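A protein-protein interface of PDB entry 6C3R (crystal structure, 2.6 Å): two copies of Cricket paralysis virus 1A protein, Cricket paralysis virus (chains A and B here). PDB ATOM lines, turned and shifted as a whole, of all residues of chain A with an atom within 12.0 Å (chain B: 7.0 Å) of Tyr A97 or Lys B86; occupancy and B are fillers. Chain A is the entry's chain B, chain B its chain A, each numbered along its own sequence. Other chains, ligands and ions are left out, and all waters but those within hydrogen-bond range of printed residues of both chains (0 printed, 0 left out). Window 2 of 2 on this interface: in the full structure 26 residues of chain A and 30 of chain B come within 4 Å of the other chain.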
ATOM      1  N   CYS A  92     -20.591 -14.626 -41.450  1.00  0.00           N
ATOM      2  CA  CYS A  92     -20.449 -14.761 -39.990  1.00  0.00           C
ATOM      3  C   CYS A  92     -20.374 -13.399 -39.302  1.00  0.00           C
ATOM      4  O   CYS A  92     -19.568 -12.560 -39.712  1.00  0.00           O
ATOM      5  CB  CYS A  92     -19.198 -15.543 -39.629  1.00  0.00           C
ATOM      6  SG  CYS A  92     -17.722 -15.071 -40.553  1.00  0.00           S
ATOM      7  N   PRO A  93     -21.191 -13.180 -38.247  1.00  0.00           N
ATOM      8  CA  PRO A  93     -21.059 -11.918 -37.494  1.00  0.00           C
ATOM      9  C   PRO A  93     -19.709 -11.796 -36.765  1.00  0.00           C
ATOM     10  O   PRO A  93     -19.132 -12.821 -36.365  1.00  0.00           O
ATOM     11  CB  PRO A  93     -22.213 -11.966 -36.478  1.00  0.00           C
ATOM     12  CG  PRO A  93     -23.015 -13.182 -36.780  1.00  0.00           C
ATOM     13  CD  PRO A  93     -22.209 -14.077 -37.666  1.00  0.00           C
ATOM     14  N   GLU A  94     -19.220 -10.561 -36.610  1.00  0.00           N
ATOM     15  CA  GLU A  94     -18.008 -10.279 -35.820  1.00  0.00           C
ATOM     16  C   GLU A  94     -18.393 -10.227 -34.338  1.00  0.00           C
ATOM     17  O   GLU A  94     -19.249  -9.423 -33.956  1.00  0.00           O
ATOM     18  CB  GLU A  94     -17.353  -8.958 -36.257  1.00  0.00           C
ATOM     19  CG  GLU A  94     -15.992  -8.684 -35.613  1.00  0.00           C
ATOM     20  CD  GLU A  94     -15.201  -7.552 -36.262  1.00  0.00           C
ATOM     21  OE1 GLU A  94     -15.631  -7.002 -37.302  1.00  0.00           O
ATOM     22  OE2 GLU A  94     -14.125  -7.212 -35.724  1.00  0.00           O
ATOM     23  N   HIS A  95     -17.773 -11.092 -33.522  1.00  0.00           N
ATOM     24  CA  HIS A  95     -18.084 -11.221 -32.086  1.00  0.00           C
ATOM     25  C   HIS A  95     -16.878 -10.865 -31.203  1.00  0.00           C
ATOM     26  O   HIS A  95     -15.848 -11.544 -31.251  1.00  0.00           O
ATOM     27  CB  HIS A  95     -18.552 -12.649 -31.757  1.00  0.00           C
ATOM     28  CG  HIS A  95     -19.885 -13.010 -32.344  1.00  0.00           C
ATOM     29  ND1 HIS A  95     -21.002 -12.208 -32.220  1.00  0.00           N
ATOM     30  CD2 HIS A  95     -20.285 -14.103 -33.039  1.00  0.00           C
ATOM     31  CE1 HIS A  95     -22.026 -12.785 -32.825  1.00  0.00           C
ATOM     32  NE2 HIS A  95     -21.618 -13.935 -33.330  1.00  0.00           N
ATOM     33  N   ARG A  96     -17.020  -9.793 -30.417  1.00  0.00           N
ATOM     34  CA  ARG A  96     -16.066  -9.425 -29.357  1.00  0.00           C
ATOM     35  C   ARG A  96     -16.826  -8.983 -28.087  1.00  0.00           C
ATOM     36  O   ARG A  96     -17.422  -7.904 -28.066  1.00  0.00           O
ATOM     37  CB  ARG A  96     -15.080  -8.338 -29.831  1.00  0.00           C
ATOM     38  CG  ARG A  96     -15.664  -7.231 -30.705  1.00  0.00           C
ATOM     39  CD  ARG A  96     -14.694  -6.063 -30.874  1.00  0.00           C
ATOM     40  NE  ARG A  96     -14.703  -5.139 -29.726  1.00  0.00           N
ATOM     41  CZ  ARG A  96     -13.845  -5.133 -28.693  1.00  0.00           C
ATOM     42  NH1 ARG A  96     -12.839  -6.005 -28.592  1.00  0.00           N
ATOM     43  NH2 ARG A  96     -13.996  -4.228 -27.732  1.00  0.00           N
ATOM     44  N   TYR A  97     -16.790  -9.832 -27.050  1.00  0.00           N
ATOM     45  CA  TYR A  97     -17.544  -9.665 -25.785  1.00  0.00           C
ATOM     46  C   TYR A  97     -19.071  -9.809 -25.967  1.00  0.00           C
ATOM     47  O   TYR A  97     -19.846  -8.949 -25.534  1.00  0.00           O
ATOM     48  CB  TYR A  97     -17.203  -8.337 -25.071  1.00  0.00           C
ATOM     49  CG  TYR A  97     -15.751  -8.159 -24.654  1.00  0.00           C
ATOM     50  CD1 TYR A  97     -14.820  -7.550 -25.506  1.00  0.00           C
ATOM     51  CD2 TYR A  97     -15.315  -8.561 -23.386  1.00  0.00           C
ATOM     52  CE1 TYR A  97     -13.497  -7.370 -25.113  1.00  0.00           C
ATOM     53  CE2 TYR A  97     -13.996  -8.386 -22.986  1.00  0.00           C
ATOM     54  CZ  TYR A  97     -13.089  -7.790 -23.849  1.00  0.00           C
ATOM     55  OH  TYR A  97     -11.786  -7.618 -23.444  1.00  0.00           O
ATOM     56  N   GLY A  98     -19.493 -10.910 -26.589  1.00  0.00           N
ATOM     57  CA  GLY A  98     -20.911 -11.156 -26.877  1.00  0.00           C
ATOM     58  C   GLY A  98     -21.441 -10.213 -27.946  1.00  0.00           C
ATOM     59  O   GLY A  98     -21.378 -10.519 -29.139  1.00  0.00           O
ATOM     60  N   SER A  99     -21.952  -9.061 -27.507  1.00  0.00           N
ATOM     61  CA  SER A  99     -22.420  -7.980 -28.398  1.00  0.00           C
ATOM     62  C   SER A  99     -21.221  -7.358 -29.149  1.00  0.00           C
ATOM     63  O   SER A  99     -20.199  -7.096 -28.511  1.00  0.00           O
ATOM     64  CB  SER A  99     -23.136  -6.908 -27.560  1.00  0.00           C
ATOM     65  OG  SER A  99     -23.503  -5.772 -28.324  1.00  0.00           O
ATOM     66  N   THR A 100     -21.306  -7.079 -30.462  1.00  0.00           N
ATOM     67  CA  THR A 100     -22.532  -7.071 -31.286  1.00  0.00           C
ATOM     68  C   THR A 100     -22.834  -8.420 -31.964  1.00  0.00           C
ATOM     69  O   THR A 100     -21.930  -9.213 -32.250  1.00  0.00           O
ATOM     70  CB  THR A 100     -22.437  -5.990 -32.403  1.00  0.00           C
ATOM     71  OG1 THR A 100     -21.837  -4.797 -31.883  1.00  0.00           O
ATOM     72  CG2 THR A 100     -23.816  -5.641 -32.988  1.00  0.00           C
ATOM     73  N   PHE A 101     -24.123  -8.648 -32.212  1.00  0.00           N
ATOM     74  CA  PHE A 101     -24.631  -9.761 -33.009  1.00  0.00           C
ATOM     75  C   PHE A 101     -25.208  -9.142 -34.306  1.00  0.00           C
ATOM     76  O   PHE A 101     -26.401  -8.815 -34.373  1.00  0.00           O
ATOM     77  CB  PHE A 101     -25.709 -10.520 -32.202  1.00  0.00           C
ATOM     78  CG  PHE A 101     -25.179 -11.670 -31.364  1.00  0.00           C
ATOM     79  CD1 PHE A 101     -24.177 -11.480 -30.415  1.00  0.00           C
ATOM     80  CD2 PHE A 101     -25.715 -12.949 -31.507  1.00  0.00           C
ATOM     81  CE1 PHE A 101     -23.713 -12.551 -29.648  1.00  0.00           C
ATOM     82  CE2 PHE A 101     -25.254 -14.016 -30.744  1.00  0.00           C
ATOM     83  CZ  PHE A 101     -24.252 -13.816 -29.812  1.00  0.00           C
ATOM     84  N   GLY A 102     -24.350  -8.967 -35.320  1.00  0.00           N
ATOM     85  CA  GLY A 102     -24.670  -8.175 -36.536  1.00  0.00           C
ATOM     86  C   GLY A 102     -25.322  -8.875 -37.732  1.00  0.00           C
ATOM     87  O   GLY A 102     -25.453 -10.105 -37.754  1.00  0.00           O
ATOM     88  N   ARG B  58      -8.452  -7.921 -36.464  1.00  0.00           N
ATOM     89  CA  ARG B  58      -8.613  -8.483 -35.127  1.00  0.00           C
ATOM     90  C   ARG B  58      -8.002  -9.892 -34.950  1.00  0.00           C
ATOM     91  O   ARG B  58      -7.351 -10.148 -33.940  1.00  0.00           O
ATOM     92  CB  ARG B  58     -10.095  -8.488 -34.762  1.00  0.00           C
ATOM     93  CG  ARG B  58     -10.436  -9.097 -33.421  1.00  0.00           C
ATOM     94  CD  ARG B  58      -9.921  -8.264 -32.259  1.00  0.00           C
ATOM     95  NE  ARG B  58     -10.662  -8.603 -31.036  1.00  0.00           N
ATOM     96  CZ  ARG B  58     -10.255  -8.380 -29.788  1.00  0.00           C
ATOM     97  NH1 ARG B  58      -9.089  -7.781 -29.528  1.00  0.00           N
ATOM     98  NH2 ARG B  58     -11.035  -8.755 -28.780  1.00  0.00           N
ATOM     99  N   LEU B  62      -4.736 -10.753 -32.425  1.00  0.00           N
ATOM    100  CA  LEU B  62      -4.851 -11.775 -31.411  1.00  0.00           C
ATOM    101  C   LEU B  62      -3.854 -12.926 -31.574  1.00  0.00           C
ATOM    102  O   LEU B  62      -3.295 -13.398 -30.583  1.00  0.00           O
ATOM    103  CB  LEU B  62      -6.286 -12.325 -31.392  1.00  0.00           C
ATOM    104  CG  LEU B  62      -7.375 -11.400 -30.852  1.00  0.00           C
ATOM    105  CD1 LEU B  62      -8.750 -11.983 -31.059  1.00  0.00           C
ATOM    106  CD2 LEU B  62      -7.147 -11.108 -29.389  1.00  0.00           C
ATOM    107  N   ILE B  66      -1.185 -13.799 -28.712  1.00  0.00           N
ATOM    108  CA  ILE B  66      -1.149 -15.144 -28.197  1.00  0.00           C
ATOM    109  C   ILE B  66       0.269 -15.676 -28.298  1.00  0.00           C
ATOM    110  O   ILE B  66       0.705 -16.421 -27.436  1.00  0.00           O
ATOM    111  CB  ILE B  66      -2.168 -16.074 -28.924  1.00  0.00           C
ATOM    112  CG1 ILE B  66      -3.596 -15.730 -28.476  1.00  0.00           C
ATOM    113  CG2 ILE B  66      -1.898 -17.572 -28.685  1.00  0.00           C
ATOM    114  CD1 ILE B  66      -4.676 -16.107 -29.480  1.00  0.00           C
ATOM    115  N   GLU B  79      -5.438 -15.345 -18.352  1.00  0.00           N
ATOM    116  CA  GLU B  79      -5.527 -14.233 -19.280  1.00  0.00           C
ATOM    117  C   GLU B  79      -5.055 -14.615 -20.663  1.00  0.00           C
ATOM    118  O   GLU B  79      -5.585 -14.144 -21.635  1.00  0.00           O
ATOM    119  CB  GLU B  79      -4.727 -13.055 -18.749  1.00  0.00           C
ATOM    120  CG  GLU B  79      -5.341 -12.482 -17.484  1.00  0.00           C
ATOM    121  CD  GLU B  79      -6.711 -11.889 -17.733  1.00  0.00           C
ATOM    122  OE1 GLU B  79      -7.630 -12.128 -16.922  1.00  0.00           O
ATOM    123  OE2 GLU B  79      -6.875 -11.174 -18.740  1.00  0.00           O
ATOM    124  N   LYS B  81      -5.461 -17.658 -21.824  1.00  0.00           N
ATOM    125  CA  LYS B  81      -6.585 -18.433 -22.319  1.00  0.00           C
ATOM    126  C   LYS B  81      -7.722 -17.588 -22.809  1.00  0.00           C
ATOM    127  O   LYS B  81      -8.357 -17.939 -23.798  1.00  0.00           O
ATOM    128  CB  LYS B  81      -7.113 -19.364 -21.261  1.00  0.00           C
ATOM    129  CG  LYS B  81      -6.310 -20.649 -21.144  1.00  0.00           C
ATOM    130  CD  LYS B  81      -6.526 -21.305 -19.792  1.00  0.00           C
ATOM    131  CE  LYS B  81      -7.975 -21.660 -19.527  1.00  0.00           C
ATOM    132  NZ  LYS B  81      -8.157 -21.911 -18.066  1.00  0.00           N
ATOM    133  N   GLY B  82      -8.000 -16.487 -22.115  1.00  0.00           N
ATOM    134  CA  GLY B  82      -9.033 -15.559 -22.561  1.00  0.00           C
ATOM    135  C   GLY B  82      -8.738 -14.990 -23.938  1.00  0.00           C
ATOM    136  O   GLY B  82      -9.656 -14.774 -24.710  1.00  0.00           O
ATOM    137  N   LEU B  83      -7.467 -14.742 -24.251  1.00  0.00           N
ATOM    138  CA  LEU B  83      -7.080 -14.302 -25.594  1.00  0.00           C
ATOM    139  C   LEU B  83      -7.375 -15.388 -26.623  1.00  0.00           C
ATOM    140  O   LEU B  83      -7.916 -15.124 -27.673  1.00  0.00           O
ATOM    141  CB  LEU B  83      -5.591 -13.955 -25.675  1.00  0.00           C
ATOM    142  CG  LEU B  83      -5.034 -12.723 -24.960  1.00  0.00           C
ATOM    143  CD1 LEU B  83      -3.520 -12.775 -24.903  1.00  0.00           C
ATOM    144  CD2 LEU B  83      -5.499 -11.465 -25.658  1.00  0.00           C
ATOM    145  N   VAL B  84      -7.041 -16.619 -26.303  1.00  0.00           N
ATOM    146  CA  VAL B  84      -7.382 -17.715 -27.188  1.00  0.00           C
ATOM    147  C   VAL B  84      -8.895 -17.766 -27.413  1.00  0.00           C
ATOM    148  O   VAL B  84      -9.356 -18.000 -28.510  1.00  0.00           O
ATOM    149  CB  VAL B  84      -6.847 -19.064 -26.655  1.00  0.00           C
ATOM    150  CG1 VAL B  84      -7.279 -20.199 -27.550  1.00  0.00           C
ATOM    151  CG2 VAL B  84      -5.328 -19.022 -26.580  1.00  0.00           C
ATOM    152  N   TRP B  85      -9.653 -17.573 -26.350  1.00  0.00           N
ATOM    153  CA  TRP B  85     -11.111 -17.589 -26.419  1.00  0.00           C
ATOM    154  C   TRP B  85     -11.660 -16.495 -27.344  1.00  0.00           C
ATOM    155  O   TRP B  85     -12.563 -16.738 -28.127  1.00  0.00           O
ATOM    156  CB  TRP B  85     -11.702 -17.489 -25.000  1.00  0.00           C
ATOM    157  CG  TRP B  85     -13.187 -17.316 -25.006  1.00  0.00           C
ATOM    158  CD1 TRP B  85     -13.894 -16.255 -24.511  1.00  0.00           C
ATOM    159  CD2 TRP B  85     -14.144 -18.216 -25.570  1.00  0.00           C
ATOM    160  NE1 TRP B  85     -15.227 -16.440 -24.738  1.00  0.00           N
ATOM    161  CE2 TRP B  85     -15.415 -17.639 -25.377  1.00  0.00           C
ATOM    162  CE3 TRP B  85     -14.052 -19.460 -26.221  1.00  0.00           C
ATOM    163  CZ2 TRP B  85     -16.594 -18.265 -25.812  1.00  0.00           C
ATOM    164  CZ3 TRP B  85     -15.215 -20.082 -26.655  1.00  0.00           C
ATOM    165  CH2 TRP B  85     -16.471 -19.484 -26.449  1.00  0.00           C
ATOM    166  N   LYS B  86     -11.101 -15.298 -27.242  1.00  0.00           N
ATOM    167  CA  LYS B  86     -11.427 -14.210 -28.176  1.00  0.00           C
ATOM    168  C   LYS B  86     -11.073 -14.500 -29.631  1.00  0.00           C
ATOM    169  O   LYS B  86     -11.797 -14.088 -30.528  1.00  0.00           O
ATOM    170  CB  LYS B  86     -10.738 -12.935 -27.772  1.00  0.00           C
ATOM    171  CG  LYS B  86     -11.371 -12.265 -26.587  1.00  0.00           C
ATOM    172  CD  LYS B  86     -10.366 -11.298 -25.993  1.00  0.00           C
ATOM    173  CE  LYS B  86     -10.991 -10.376 -24.980  1.00  0.00           C
ATOM    174  NZ  LYS B  86      -9.893  -9.807 -24.146  1.00  0.00           N
ATOM    175  N   PHE B  87      -9.941 -15.156 -29.853  1.00  0.00           N
ATOM    176  CA  PHE B  87      -9.564 -15.634 -31.179  1.00  0.00           C
ATOM    177  C   PHE B  87     -10.605 -16.621 -31.670  1.00  0.00           C
ATOM    178  O   PHE B  87     -11.151 -16.443 -32.741  1.00  0.00           O
ATOM    179  CB  PHE B  87      -8.180 -16.292 -31.161  1.00  0.00           C
ATOM    180  CG  PHE B  87      -7.707 -16.731 -32.507  1.00  0.00           C
ATOM    181  CD1 PHE B  87      -8.014 -17.999 -32.985  1.00  0.00           C
ATOM    182  CD2 PHE B  87      -6.967 -15.877 -33.309  1.00  0.00           C
ATOM    183  CE1 PHE B  87      -7.604 -18.422 -34.249  1.00  0.00           C
ATOM    184  CE2 PHE B  87      -6.530 -16.293 -34.561  1.00  0.00           C
ATOM    185  CZ  PHE B  87      -6.868 -17.568 -35.042  1.00  0.00           C
ATOM    186  N   VAL B  88     -10.856 -17.656 -30.881  1.00  0.00           N
ATOM    187  CA  VAL B  88     -11.865 -18.671 -31.173  1.00  0.00           C
ATOM    188  C   VAL B  88     -13.236 -18.030 -31.453  1.00  0.00           C
ATOM    189  O   VAL B  88     -13.878 -18.387 -32.420  1.00  0.00           O
ATOM    190  CB  VAL B  88     -11.938 -19.705 -30.023  1.00  0.00           C
ATOM    191  CG1 VAL B  88     -13.242 -20.476 -30.015  1.00  0.00           C
ATOM    192  CG2 VAL B  88     -10.779 -20.690 -30.125  1.00  0.00           C
ATOM    193  N   GLN B  89     -13.672 -17.074 -30.635  1.00  0.00           N
ATOM    194  CA  GLN B  89     -14.910 -16.330 -30.922  1.00  0.00           C
ATOM    195  C   GLN B  89     -14.865 -15.630 -32.289  1.00  0.00           C
ATOM    196  O   GLN B  89     -15.805 -15.711 -33.069  1.00  0.00           O
ATOM    197  CB  GLN B  89     -15.203 -15.281 -29.849  1.00  0.00           C
ATOM    198  CG  GLN B  89     -15.808 -15.848 -28.579  1.00  0.00           C
ATOM    199  CD  GLN B  89     -16.285 -14.775 -27.592  1.00  0.00           C
ATOM    200  OE1 GLN B  89     -16.869 -15.106 -26.548  1.00  0.00           O
ATOM    201  NE2 GLN B  89     -16.048 -13.490 -27.909  1.00  0.00           N
ATOM    202  N   ASN B  90     -13.767 -14.948 -32.569  1.00  0.00           N
ATOM    203  CA  ASN B  90     -13.632 -14.221 -33.813  1.00  0.00           C
ATOM    204  C   ASN B  90     -13.392 -15.118 -35.044  1.00  0.00           C
ATOM    205  O   ASN B  90     -13.635 -14.698 -36.171  1.00  0.00           O
ATOM    206  CB  ASN B  90     -12.534 -13.163 -33.683  1.00  0.00           C
ATOM    207  CG  ASN B  90     -12.756 -11.967 -34.596  1.00  0.00           C
ATOM    208  OD1 ASN B  90     -13.799 -11.291 -34.532  1.00  0.00           O
ATOM    209  ND2 ASN B  90     -11.775 -11.683 -35.438  1.00  0.00           N
ATOM    210  N   TYR B  91     -12.910 -16.340 -34.848  1.00  0.00           N
ATOM    211  CA  TYR B  91     -12.693 -17.222 -35.992  1.00  0.00           C
ATOM    212  C   TYR B  91     -14.036 -17.656 -36.613  1.00  0.00           C
ATOM    213  O   TYR B  91     -15.054 -17.758 -35.945  1.00  0.00           O
ATOM    214  CB  TYR B  91     -11.801 -18.423 -35.637  1.00  0.00           C
ATOM    215  CG  TYR B  91     -11.476 -19.312 -36.829  1.00  0.00           C
ATOM    216  CD1 TYR B  91     -10.521 -18.940 -37.776  1.00  0.00           C
ATOM    217  CD2 TYR B  91     -12.144 -20.507 -37.021  1.00  0.00           C
ATOM    218  CE1 TYR B  91     -10.234 -19.750 -38.873  1.00  0.00           C
ATOM    219  CE2 TYR B  91     -11.870 -21.322 -38.098  1.00  0.00           C
ATOM    220  CZ  TYR B  91     -10.920 -20.948 -39.034  1.00  0.00           C
ATOM    221  OH  TYR B  91     -10.670 -21.797 -40.115  1.00  0.00           O
ATOM    222  N   LEU B 136     -11.766 -23.046 -22.033  1.00  0.00           N
ATOM    223  CA  LEU B 136     -11.081 -21.740 -21.992  1.00  0.00           C
ATOM    224  C   LEU B 136     -11.586 -20.713 -20.946  1.00  0.00           C
ATOM    225  O   LEU B 136     -11.053 -19.599 -20.890  1.00  0.00           O
ATOM    226  CB  LEU B 136     -11.084 -21.099 -23.389  1.00  0.00           C
ATOM    227  CG  LEU B 136     -10.456 -21.911 -24.531  1.00  0.00           C
ATOM    228  CD1 LEU B 136     -10.662 -21.168 -25.847  1.00  0.00           C
ATOM    229  CD2 LEU B 136      -8.974 -22.212 -24.291  1.00  0.00           C
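OE1 of Gln B89 is in hydrogen-bond range of NE1 of Trp B85 (2.8 Å).
ND1 of His A95 is in hydrogen-bond range of O of Thr A100 (3.1 Å).
No position is printed for both chains.
The side-chain amino group of Lys B86 sits at hydrogen-bond distance from the side-chain hydroxyl of Tyr A97, at 3.0 Å.
The guanidinium group (NH1) of Arg A96 sits close to the guanidinium group (NH2) of Arg B58 (3.3 Å).
Among the printed residues, pairs that only touch across the chains: Glu A94 with Asn B90 (3.6 Å), Tyr A97 with Gln B89 (3.8 Å), His A95 with Gln B89 (3.9 Å) and His A95 with Asn B90 (3.9 Å).
Of the 11 printed residues of chain A, 4 touch a printed residue of chain B.
Printed residues of chain A that touch a printed residue of chain B: Glu A94, His A95, Arg A96 and Tyr A97.
Along chain B the printed residues that touch a printed residue of chain A span positions 58 to 90.
Printed residues of chain B within 4 Å of Glu A94: Asn B90 (3.6 Å).
Of the printed residues of chain B, Arg A96 touches Arg B58.
Tyr A97 touches just these residues of chain B: Lys B86 and Gln B89.
Of the printed residues of chain A, Arg B58 touches Arg A96 (3.3 Å).
No residue of chain A comes within 4 Å of Leu B62.
Ile B66 touches none of the printed residues of chain A.
Lys B81 touches none of the printed residues of chain A.
No residue of chain A comes within 4 Å of Gly B82.
Leu B83 touches none of the printed residues of chain A.
Of the printed residues of chain A, Lys B86 touches Tyr A97.
No residue of chain A comes within 4 Å of Phe B87.
Of chain A, only Glu A94 (3.6 Å) and His A95 (3.9 Å) come within 4 Å of Asn B90.
The nearest residue of chain B that does not touch Tyr A97 is Arg B58 (4.6 Å).
The nearest residue of chain A that does not touch Lys B86 is His A95 (4.8 Å).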
